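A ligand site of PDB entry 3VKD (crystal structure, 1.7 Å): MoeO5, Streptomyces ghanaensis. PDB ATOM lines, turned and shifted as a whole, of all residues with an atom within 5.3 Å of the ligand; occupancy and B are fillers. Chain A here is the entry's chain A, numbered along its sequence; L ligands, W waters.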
ATOM      1  N   ILE A  44       9.363  13.606 -10.894  1.00  0.00           N
ATOM      2  CA  ILE A  44       9.515  12.692 -12.006  1.00  0.00           C
ATOM      3  C   ILE A  44      10.987  12.687 -12.390  1.00  0.00           C
ATOM      4  O   ILE A  44      11.526  13.703 -12.760  1.00  0.00           O
ATOM      5  CB  ILE A  44       8.686  13.180 -13.206  1.00  0.00           C
ATOM      6  CG1 ILE A  44       7.207  13.191 -12.799  1.00  0.00           C
ATOM      7  CG2 ILE A  44       8.922  12.258 -14.383  1.00  0.00           C
ATOM      8  CD1 ILE A  44       6.360  14.134 -13.704  1.00  0.00           C
ATOM      9  N   ALA A  73      10.120   8.722 -15.987  1.00  0.00           N
ATOM     10  CA  ALA A  73       9.432   9.003 -17.253  1.00  0.00           C
ATOM     11  C   ALA A  73      10.287   9.767 -18.204  1.00  0.00           C
ATOM     12  O   ALA A  73      11.111  10.555 -17.783  1.00  0.00           O
ATOM     13  CB  ALA A  73       8.137   9.832 -16.945  1.00  0.00           C
ATOM     14  N   SER A  74      10.086   9.534 -19.497  1.00  0.00           N
ATOM     15  CA  SER A  74      10.804  10.289 -20.516  1.00  0.00           C
ATOM     16  C   SER A  74      10.054  10.113 -21.831  1.00  0.00           C
ATOM     17  O   SER A  74       9.432   9.076 -22.065  1.00  0.00           O
ATOM     18  CB  SER A  74      12.226   9.707 -20.734  1.00  0.00           C
ATOM     19  OG  SER A  74      12.859  10.550 -21.724  1.00  0.00           O
ATOM     20  N   THR A  75      10.178  11.106 -22.716  1.00  0.00           N
ATOM     21  CA  THR A  75       9.619  10.962 -24.054  1.00  0.00           C
ATOM     22  C   THR A  75      10.558  10.055 -24.888  1.00  0.00           C
ATOM     23  O   THR A  75      10.134   9.241 -25.752  1.00  0.00           O
ATOM     24  CB  THR A  75       9.534  12.371 -24.742  1.00  0.00           C
ATOM     25  OG1 THR A  75       8.629  13.226 -23.976  1.00  0.00           O
ATOM     26  CG2 THR A  75       9.008  12.229 -26.128  1.00  0.00           C
ATOM     27  N   HIS A 102       6.556   5.743 -16.874  1.00  0.00           N
ATOM     28  CA  HIS A 102       5.657   6.425 -17.830  1.00  0.00           C
ATOM     29  C   HIS A 102       6.439   6.780 -19.106  1.00  0.00           C
ATOM     30  O   HIS A 102       7.280   7.719 -19.112  1.00  0.00           O
ATOM     31  CB  HIS A 102       5.087   7.706 -17.198  1.00  0.00           C
ATOM     32  CG  HIS A 102       4.039   8.340 -18.045  1.00  0.00           C
ATOM     33  ND1 HIS A 102       3.649   9.637 -17.875  1.00  0.00           N
ATOM     34  CD2 HIS A 102       3.283   7.828 -19.065  1.00  0.00           C
ATOM     35  CE1 HIS A 102       2.667   9.910 -18.737  1.00  0.00           C
ATOM     36  NE2 HIS A 102       2.430   8.829 -19.465  1.00  0.00           N
ATOM     37  N   PHE A 103       6.174   6.043 -20.207  1.00  0.00           N
ATOM     38  CA  PHE A 103       6.902   6.244 -21.463  1.00  0.00           C
ATOM     39  C   PHE A 103       5.909   6.013 -22.610  1.00  0.00           C
ATOM     40  O   PHE A 103       4.932   5.320 -22.438  1.00  0.00           O
ATOM     41  CB  PHE A 103       8.019   5.176 -21.617  1.00  0.00           C
ATOM     42  CG  PHE A 103       9.095   5.279 -20.547  1.00  0.00           C
ATOM     43  CD1 PHE A 103       8.927   4.633 -19.347  1.00  0.00           C
ATOM     44  CD2 PHE A 103      10.183   6.124 -20.732  1.00  0.00           C
ATOM     45  CE1 PHE A 103       9.847   4.829 -18.300  1.00  0.00           C
ATOM     46  CE2 PHE A 103      11.125   6.335 -19.665  1.00  0.00           C
ATOM     47  CZ  PHE A 103      10.913   5.676 -18.487  1.00  0.00           C
ATOM     48  N   PRO A 104       6.171   6.598 -23.775  1.00  0.00           N
ATOM     49  CA  PRO A 104       5.268   6.399 -24.896  1.00  0.00           C
ATOM     50  C   PRO A 104       5.507   5.005 -25.471  1.00  0.00           C
ATOM     51  O   PRO A 104       6.571   4.408 -25.319  1.00  0.00           O
ATOM     52  CB  PRO A 104       5.680   7.482 -25.918  1.00  0.00           C
ATOM     53  CG  PRO A 104       7.187   7.686 -25.605  1.00  0.00           C
ATOM     54  CD  PRO A 104       7.213   7.611 -24.044  1.00  0.00           C
ATOM     55  N   PRO A 123      -0.730   5.672 -20.990  1.00  0.00           N
ATOM     56  CA  PRO A 123      -1.479   6.821 -21.491  1.00  0.00           C
ATOM     57  C   PRO A 123      -2.276   6.541 -22.765  1.00  0.00           C
ATOM     58  O   PRO A 123      -1.667   6.136 -23.757  1.00  0.00           O
ATOM     59  CB  PRO A 123      -0.369   7.874 -21.800  1.00  0.00           C
ATOM     60  CG  PRO A 123       0.868   7.006 -22.109  1.00  0.00           C
ATOM     61  CD  PRO A 123       0.737   5.851 -21.113  1.00  0.00           C
ATOM     62  N   LEU A 125      -3.906   8.451 -25.473  1.00  0.00           N
ATOM     63  CA  LEU A 125      -3.800   9.865 -25.936  1.00  0.00           C
ATOM     64  C   LEU A 125      -5.043  10.205 -26.760  1.00  0.00           C
ATOM     65  O   LEU A 125      -5.029  10.157 -28.004  1.00  0.00           O
ATOM     66  CB  LEU A 125      -2.486  10.010 -26.732  1.00  0.00           C
ATOM     67  CG  LEU A 125      -1.279   9.851 -25.760  1.00  0.00           C
ATOM     68  CD1 LEU A 125      -0.081   9.235 -26.478  1.00  0.00           C
ATOM     69  CD2 LEU A 125      -0.899  11.218 -25.238  1.00  0.00           C
ATOM     70  N   ALA A 162      -4.615  10.638 -21.295  1.00  0.00           N
ATOM     71  CA  ALA A 162      -3.463  11.581 -21.368  1.00  0.00           C
ATOM     72  C   ALA A 162      -3.772  12.621 -22.380  1.00  0.00           C
ATOM     73  O   ALA A 162      -4.038  12.284 -23.527  1.00  0.00           O
ATOM     74  CB  ALA A 162      -2.162  10.791 -21.768  1.00  0.00           C
ATOM     75  N   LEU A 163      -3.693  13.882 -21.965  1.00  0.00           N
ATOM     76  CA  LEU A 163      -4.072  15.022 -22.800  1.00  0.00           C
ATOM     77  C   LEU A 163      -2.951  16.046 -22.816  1.00  0.00           C
ATOM     78  O   LEU A 163      -2.315  16.254 -21.798  1.00  0.00           O
ATOM     79  CB  LEU A 163      -5.340  15.650 -22.207  1.00  0.00           C
ATOM     80  CG  LEU A 163      -6.512  14.663 -22.228  1.00  0.00           C
ATOM     81  CD1 LEU A 163      -7.728  15.398 -21.609  1.00  0.00           C
ATOM     82  CD2 LEU A 163      -6.861  14.238 -23.701  1.00  0.00           C
ATOM     83  N   THR A 164      -2.791  16.729 -23.950  1.00  0.00           N
ATOM     84  CA  THR A 164      -1.685  17.658 -24.068  1.00  0.00           C
ATOM     85  C   THR A 164      -2.210  19.062 -24.300  1.00  0.00           C
ATOM     86  O   THR A 164      -3.224  19.265 -24.999  1.00  0.00           O
ATOM     87  CB  THR A 164      -0.734  17.281 -25.243  1.00  0.00           C
ATOM     88  OG1 THR A 164      -1.405  17.354 -26.518  1.00  0.00           O
ATOM     89  CG2 THR A 164      -0.203  15.871 -25.056  1.00  0.00           C
ATOM     90  N   THR A 171       5.643  16.370 -29.275  1.00  0.00           N
ATOM     91  CA  THR A 171       4.680  15.297 -29.037  1.00  0.00           C
ATOM     92  C   THR A 171       3.771  15.096 -30.224  1.00  0.00           C
ATOM     93  O   THR A 171       3.356  13.966 -30.557  1.00  0.00           O
ATOM     94  CB  THR A 171       3.823  15.552 -27.806  1.00  0.00           C
ATOM     95  OG1 THR A 171       4.678  15.974 -26.750  1.00  0.00           O
ATOM     96  CG2 THR A 171       3.138  14.260 -27.357  1.00  0.00           C
ATOM     97  N   LEU A 175       3.683  11.394 -31.511  1.00  0.00           N
ATOM     98  CA  LEU A 175       2.463  10.676 -31.074  1.00  0.00           C
ATOM     99  C   LEU A 175       1.171  11.109 -31.709  1.00  0.00           C
ATOM    100  O   LEU A 175       0.132  10.539 -31.448  1.00  0.00           O
ATOM    101  CB  LEU A 175       2.344  10.809 -29.524  1.00  0.00           C
ATOM    102  CG  LEU A 175       3.646  10.596 -28.751  1.00  0.00           C
ATOM    103  CD1 LEU A 175       3.306  10.716 -27.262  1.00  0.00           C
ATOM    104  CD2 LEU A 175       4.226   9.138 -29.015  1.00  0.00           C
ATOM    105  N   TYR A 204      -4.158  12.423 -16.952  1.00  0.00           N
ATOM    106  CA  TYR A 204      -2.853  13.095 -16.865  1.00  0.00           C
ATOM    107  C   TYR A 204      -2.921  14.285 -17.836  1.00  0.00           C
ATOM    108  O   TYR A 204      -3.042  14.085 -19.061  1.00  0.00           O
ATOM    109  CB  TYR A 204      -1.779  12.099 -17.280  1.00  0.00           C
ATOM    110  CG  TYR A 204      -0.383  12.457 -16.852  1.00  0.00           C
ATOM    111  CD1 TYR A 204       0.312  13.469 -17.500  1.00  0.00           C
ATOM    112  CD2 TYR A 204       0.209  11.793 -15.776  1.00  0.00           C
ATOM    113  CE1 TYR A 204       1.604  13.829 -17.077  1.00  0.00           C
ATOM    114  CE2 TYR A 204       1.481  12.135 -15.341  1.00  0.00           C
ATOM    115  CZ  TYR A 204       2.153  13.150 -15.992  1.00  0.00           C
ATOM    116  OH  TYR A 204       3.437  13.474 -15.562  1.00  0.00           O
ATOM    117  N   TYR A 206      -0.978  17.377 -19.361  1.00  0.00           N
ATOM    118  CA  TYR A 206       0.427  17.733 -19.537  1.00  0.00           C
ATOM    119  C   TYR A 206       0.623  18.878 -20.516  1.00  0.00           C
ATOM    120  O   TYR A 206      -0.083  18.982 -21.516  1.00  0.00           O
ATOM    121  CB  TYR A 206       1.130  16.495 -20.110  1.00  0.00           C
ATOM    122  CG  TYR A 206       2.510  16.751 -20.715  1.00  0.00           C
ATOM    123  CD1 TYR A 206       3.594  17.113 -19.914  1.00  0.00           C
ATOM    124  CD2 TYR A 206       2.713  16.565 -22.099  1.00  0.00           C
ATOM    125  CE1 TYR A 206       4.888  17.281 -20.489  1.00  0.00           C
ATOM    126  CE2 TYR A 206       3.980  16.727 -22.680  1.00  0.00           C
ATOM    127  CZ  TYR A 206       5.052  17.066 -21.868  1.00  0.00           C
ATOM    128  OH  TYR A 206       6.303  17.160 -22.445  1.00  0.00           O
ATOM    129  N   SER A 207       1.589  19.763 -20.220  1.00  0.00           N
ATOM    130  CA  SER A 207       1.948  20.794 -21.226  1.00  0.00           C
ATOM    131  C   SER A 207       3.480  20.766 -21.340  1.00  0.00           C
ATOM    132  O   SER A 207       4.187  21.100 -20.362  1.00  0.00           O
ATOM    133  CB  SER A 207       1.526  22.188 -20.788  1.00  0.00           C
ATOM    134  OG  SER A 207       1.852  23.129 -21.854  1.00  0.00           O
ATOM    135  N   ARG A 208       3.980  20.432 -22.528  1.00  0.00           N
ATOM    136  CA  ARG A 208       5.441  20.410 -22.726  1.00  0.00           C
ATOM    137  C   ARG A 208       6.042  21.823 -22.648  1.00  0.00           C
ATOM    138  O   ARG A 208       7.089  22.035 -21.963  1.00  0.00           O
ATOM    139  CB  ARG A 208       5.788  19.855 -24.105  1.00  0.00           C
ATOM    140  CG  ARG A 208       7.341  19.621 -24.185  1.00  0.00           C
ATOM    141  CD  ARG A 208       7.788  19.016 -25.534  1.00  0.00           C
ATOM    142  NE  ARG A 208       7.260  17.657 -25.689  1.00  0.00           N
ATOM    143  CZ  ARG A 208       7.805  16.572 -25.164  1.00  0.00           C
ATOM    144  NH1 ARG A 208       8.929  16.672 -24.421  1.00  0.00           N
ATOM    145  NH2 ARG A 208       7.179  15.404 -25.328  1.00  0.00           N
ATOM    146  N   SER A 233       1.059  18.044 -15.108  1.00  0.00           N
ATOM    147  CA  SER A 233       2.530  18.316 -15.110  1.00  0.00           C
ATOM    148  C   SER A 233       2.881  19.174 -16.300  1.00  0.00           C
ATOM    149  O   SER A 233       2.071  19.371 -17.228  1.00  0.00           O
ATOM    150  CB  SER A 233       3.420  17.050 -15.191  1.00  0.00           C
ATOM    151  OG  SER A 233       3.533  16.585 -16.509  1.00  0.00           O
ATOM    152  N   GLY A 234       4.110  19.680 -16.243  1.00  0.00           N
ATOM    153  CA  GLY A 234       4.683  20.468 -17.306  1.00  0.00           C
ATOM    154  C   GLY A 234       5.040  21.857 -16.800  1.00  0.00           C
ATOM    155  O   GLY A 234       4.187  22.668 -16.495  1.00  0.00           O
ATOM    156  N   ASN A 235       6.316  22.110 -16.775  1.00  0.00           N
ATOM    157  CA  ASN A 235       6.805  23.438 -16.369  1.00  0.00           C
ATOM    158  C   ASN A 235       6.442  23.925 -14.985  1.00  0.00           C
ATOM    159  O   ASN A 235       6.314  25.148 -14.758  1.00  0.00           O
ATOM    160  CB  ASN A 235       6.433  24.459 -17.472  1.00  0.00           C
ATOM    161  CG  ASN A 235       7.032  24.050 -18.790  1.00  0.00           C
ATOM    162  OD1 ASN A 235       8.275  23.887 -18.914  1.00  0.00           O
ATOM    163  ND2 ASN A 235       6.194  23.831 -19.790  1.00  0.00           N
ATOM    164  N   VAL A 236       6.277  22.975 -14.058  1.00  0.00           N
ATOM    165  CA  VAL A 236       6.031  23.327 -12.674  1.00  0.00           C
ATOM    166  C   VAL A 236       7.411  23.520 -12.062  1.00  0.00           C
ATOM    167  O   VAL A 236       8.212  22.598 -11.953  1.00  0.00           O
ATOM    168  CB  VAL A 236       5.294  22.210 -11.909  1.00  0.00           C
ATOM    169  CG1 VAL A 236       5.222  22.526 -10.381  1.00  0.00           C
ATOM    170  CG2 VAL A 236       3.908  22.029 -12.539  1.00  0.00           C
ATOM    171  N   GLY A 254       3.105  16.949 -11.096  1.00  0.00           N
ATOM    172  CA  GLY A 254       4.408  16.374 -11.416  1.00  0.00           C
ATOM    173  C   GLY A 254       5.414  17.419 -11.841  1.00  0.00           C
ATOM    174  O   GLY A 254       5.038  18.474 -12.361  1.00  0.00           O
ATOM    175  N   PHE A 255       6.683  17.143 -11.592  1.00  0.00           N
ATOM    176  CA  PHE A 255       7.735  18.069 -12.011  1.00  0.00           C
ATOM    177  C   PHE A 255       9.024  17.274 -12.167  1.00  0.00           C
ATOM    178  O   PHE A 255       9.339  16.423 -11.354  1.00  0.00           O
ATOM    179  CB  PHE A 255       7.938  19.218 -10.951  1.00  0.00           C
ATOM    180  CG  PHE A 255       8.380  18.746  -9.601  1.00  0.00           C
ATOM    181  CD1 PHE A 255       7.494  18.137  -8.726  1.00  0.00           C
ATOM    182  CD2 PHE A 255       9.733  18.934  -9.189  1.00  0.00           C
ATOM    183  CE1 PHE A 255       7.878  17.694  -7.471  1.00  0.00           C
ATOM    184  CE2 PHE A 255      10.146  18.499  -7.905  1.00  0.00           C
ATOM    185  CZ  PHE A 255       9.232  17.883  -7.059  1.00  0.00           C
ATOM    186  N   ALA A 256       9.667  17.496 -13.299  1.00  0.00           N
ATOM    187  CA  ALA A 256      10.908  16.795 -13.621  1.00  0.00           C
ATOM    188  C   ALA A 256      12.026  17.827 -13.785  1.00  0.00           C
ATOM    189  O   ALA A 256      12.953  17.881 -12.983  1.00  0.00           O
ATOM    190  CB  ALA A 256      10.759  15.980 -14.926  1.00  0.00           C
ATOM    191  N   GLY A 257      11.865  18.684 -14.787  1.00  0.00           N
ATOM    192  CA  GLY A 257      12.926  19.635 -15.109  1.00  0.00           C
ATOM    193  C   GLY A 257      13.464  20.540 -14.021  1.00  0.00           C
ATOM    194  O   GLY A 257      14.657  20.815 -14.044  1.00  0.00           O
ATOM    195  N   ALA A 258      12.632  20.948 -13.096  1.00  0.00           N
ATOM    196  CA  ALA A 258      13.090  21.839 -12.037  1.00  0.00           C
ATOM    197  C   ALA A 258      14.252  21.191 -11.285  1.00  0.00           C
ATOM    198  O   ALA A 258      15.069  21.934 -10.731  1.00  0.00           O
ATOM    199  CB  ALA A 258      11.964  22.137 -11.059  1.00  0.00           C
HETATM  200  P1  LIG L   1       8.682  19.107 -16.673  1.00  0.00           P
HETATM  201  C1  LIG L   1       7.828  14.463 -19.969  1.00  0.00           C
HETATM  202  C2  LIG L   1       6.355  14.254 -20.235  1.00  0.00           C
HETATM  203  C3  LIG L   1       5.756  13.079 -20.096  1.00  0.00           C
HETATM  204  C4  LIG L   1       4.304  13.103 -20.348  1.00  0.00           C
HETATM  205  C5  LIG L   1       6.393  11.766 -19.662  1.00  0.00           C
HETATM  206  C6  LIG L   1       6.786  10.982 -20.936  1.00  0.00           C
HETATM  207  C7  LIG L   1       5.581  10.162 -21.407  1.00  0.00           C
HETATM  208  C8  LIG L   1       5.005  10.273 -22.621  1.00  0.00           C
HETATM  209  C9  LIG L   1       5.450  11.241 -23.712  1.00  0.00           C
HETATM  210  C10 LIG L   1       7.439  16.761 -16.777  1.00  0.00           C
HETATM  211  O1  LIG L   1       7.697  17.980 -17.428  1.00  0.00           O
HETATM  212  C11 LIG L   1       6.975  15.785 -17.890  1.00  0.00           C
HETATM  213  O2  LIG L   1       7.994  15.455 -18.768  1.00  0.00           O
HETATM  214  C12 LIG L   1       6.361  14.564 -17.145  1.00  0.00           C
HETATM  215  C13 LIG L   1       3.824   9.340 -22.936  1.00  0.00           C
HETATM  216  C14 LIG L   1       2.575  10.037 -23.489  1.00  0.00           C
HETATM  217  C15 LIG L   1       1.923  10.918 -22.436  1.00  0.00           C
HETATM  218  C16 LIG L   1       1.642  12.206 -22.500  1.00  0.00           C
HETATM  219  C17 LIG L   1       1.942  13.117 -23.711  1.00  0.00           C
HETATM  220  C18 LIG L   1       0.984  12.885 -21.328  1.00  0.00           C
HETATM  221  O3  LIG L   1       8.402  19.116 -15.216  1.00  0.00           O
HETATM  222  O4  LIG L   1       5.186  14.675 -16.729  1.00  0.00           O
HETATM  223  O5  LIG L   1      10.173  18.832 -16.992  1.00  0.00           O
HETATM  224  O6  LIG L   1       7.059  13.526 -17.031  1.00  0.00           O
HETATM  225  O7  LIG L   1       8.234  20.358 -17.412  1.00  0.00           O
HETATM  226  O   HOH W   1       8.361  17.729 -20.768  1.00  0.00           O
HETATM  227  O   HOH W   2       6.073  20.027 -14.372  1.00  0.00           O
HETATM  228  O   HOH W   3       8.333  20.387 -20.123  1.00  0.00           O
HETATM  229  O   HOH W   4       5.247  11.372 -16.119  1.00  0.00           O
HETATM  230  O   HOH W   5      11.534  20.005 -18.942  1.00  0.00           O
HETATM  231  O   HOH W   6       9.703  21.045 -13.726  1.00  0.00           O
HETATM  232  O   HOH W   7       9.906  13.269 -17.573  1.00  0.00           O
HETATM  233  O   HOH W   8      10.202  22.534 -16.114  1.00  0.00           O
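OH of Tyr 204 sits at hydrogen-bond distance from OG of Ser 233 (3.3 Å). The backbone NH (N) of Leu 163 is in hydrogen-bond range of the backbone carbonyl oxygen (O) of Tyr 204, at 3.0 Å. ND2 of Asn 235 sits at hydrogen-bond distance from O of Arg 208, at 3.0 Å. The backbone carbonyl oxygen (O) of Ser 207 is in hydrogen-bond range of the side-chain amide nitrogen (ND2) of Asn 235 (3.4 Å). The backbone carbonyl oxygen of Phe 255 lies within hydrogen-bond range of the backbone NH of Ile 44 (2.9 Å). The backbone carbonyl oxygen (O) of Leu 163 sits at hydrogen-bond distance from the backbone NH (N) of Tyr 206. NH1 of Arg 208 lies close to OH of Tyr 206 (3.3 Å). The side-chain hydroxyl (OG1) of Thr 75 lies within hydrogen-bond range of the guanidinium group (NH2) of Arg 208 (2.9 Å).
OH of Tyr 204 sits at hydrogen-bond distance from O4 of the ligand (2.4 Å). The side-chain hydroxyl (OG) of Ser 233 sits at hydrogen-bond distance from an oxygen (O4) of the ligand (2.5 Å). N of Asn 235 sits at hydrogen-bond distance from O7 of the ligand (2.7 Å). The backbone NH (N) of Gly 257 sits at hydrogen-bond distance from an oxygen (O5) of the ligand, 2.8 Å away. The backbone NH (N) of Ala 256 is in hydrogen-bond range of an oxygen (O3) of the ligand, 2.8 Å away.
Merely in contact with the ligand: Ile 44 (3.3 Å), Tyr 206 (3.4 Å), Phe 255 (3.4 Å), Ser 74 (3.5 Å), Gly 234 (3.6 Å), His 102 (3.7 Å), Pro 104 (3.7 Å), Thr 164 (3.7 Å), Pro 123 (3.7 Å), Leu 125 (3.7 Å), Thr 75 (3.8 Å), Ala 73 (3.8 Å), Ala 162 (3.8 Å), Leu 175 (3.9 Å) and Phe 103 (3.9 Å). Hydrophobic or aromatic side chains that line the ligand: Ile 44, Ala 73, His 102, Pro 104, Pro 123, Leu 125, Ala 162, Leu 175, Tyr 204, Tyr 206 and Ala 256. Of the 27 residues printed, 20 come within 4 Å of the ligand.
Water W3 bridges an oxygen (O7) of the ligand (2.7 Å) and the backbone carbonyl oxygen (O) of Arg 208 (2.8 Å). Water W6 lies within hydrogen-bond range of O3 of the ligand, O of Val 236, N of Ala 258 and N of Gly 257. Water W7 lies within hydrogen-bond range of an oxygen (O6) of the ligand (2.9 Å) and the backbone carbonyl oxygen of Ala 73 (3.0 Å). Water W4 lies within hydrogen-bond range of OH of Tyr 204, ND1 of His 102 and O6 of the ligand. Water W1 bridges OH of Tyr 206 (2.7 Å) and O2 of the ligand (3.1 Å).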
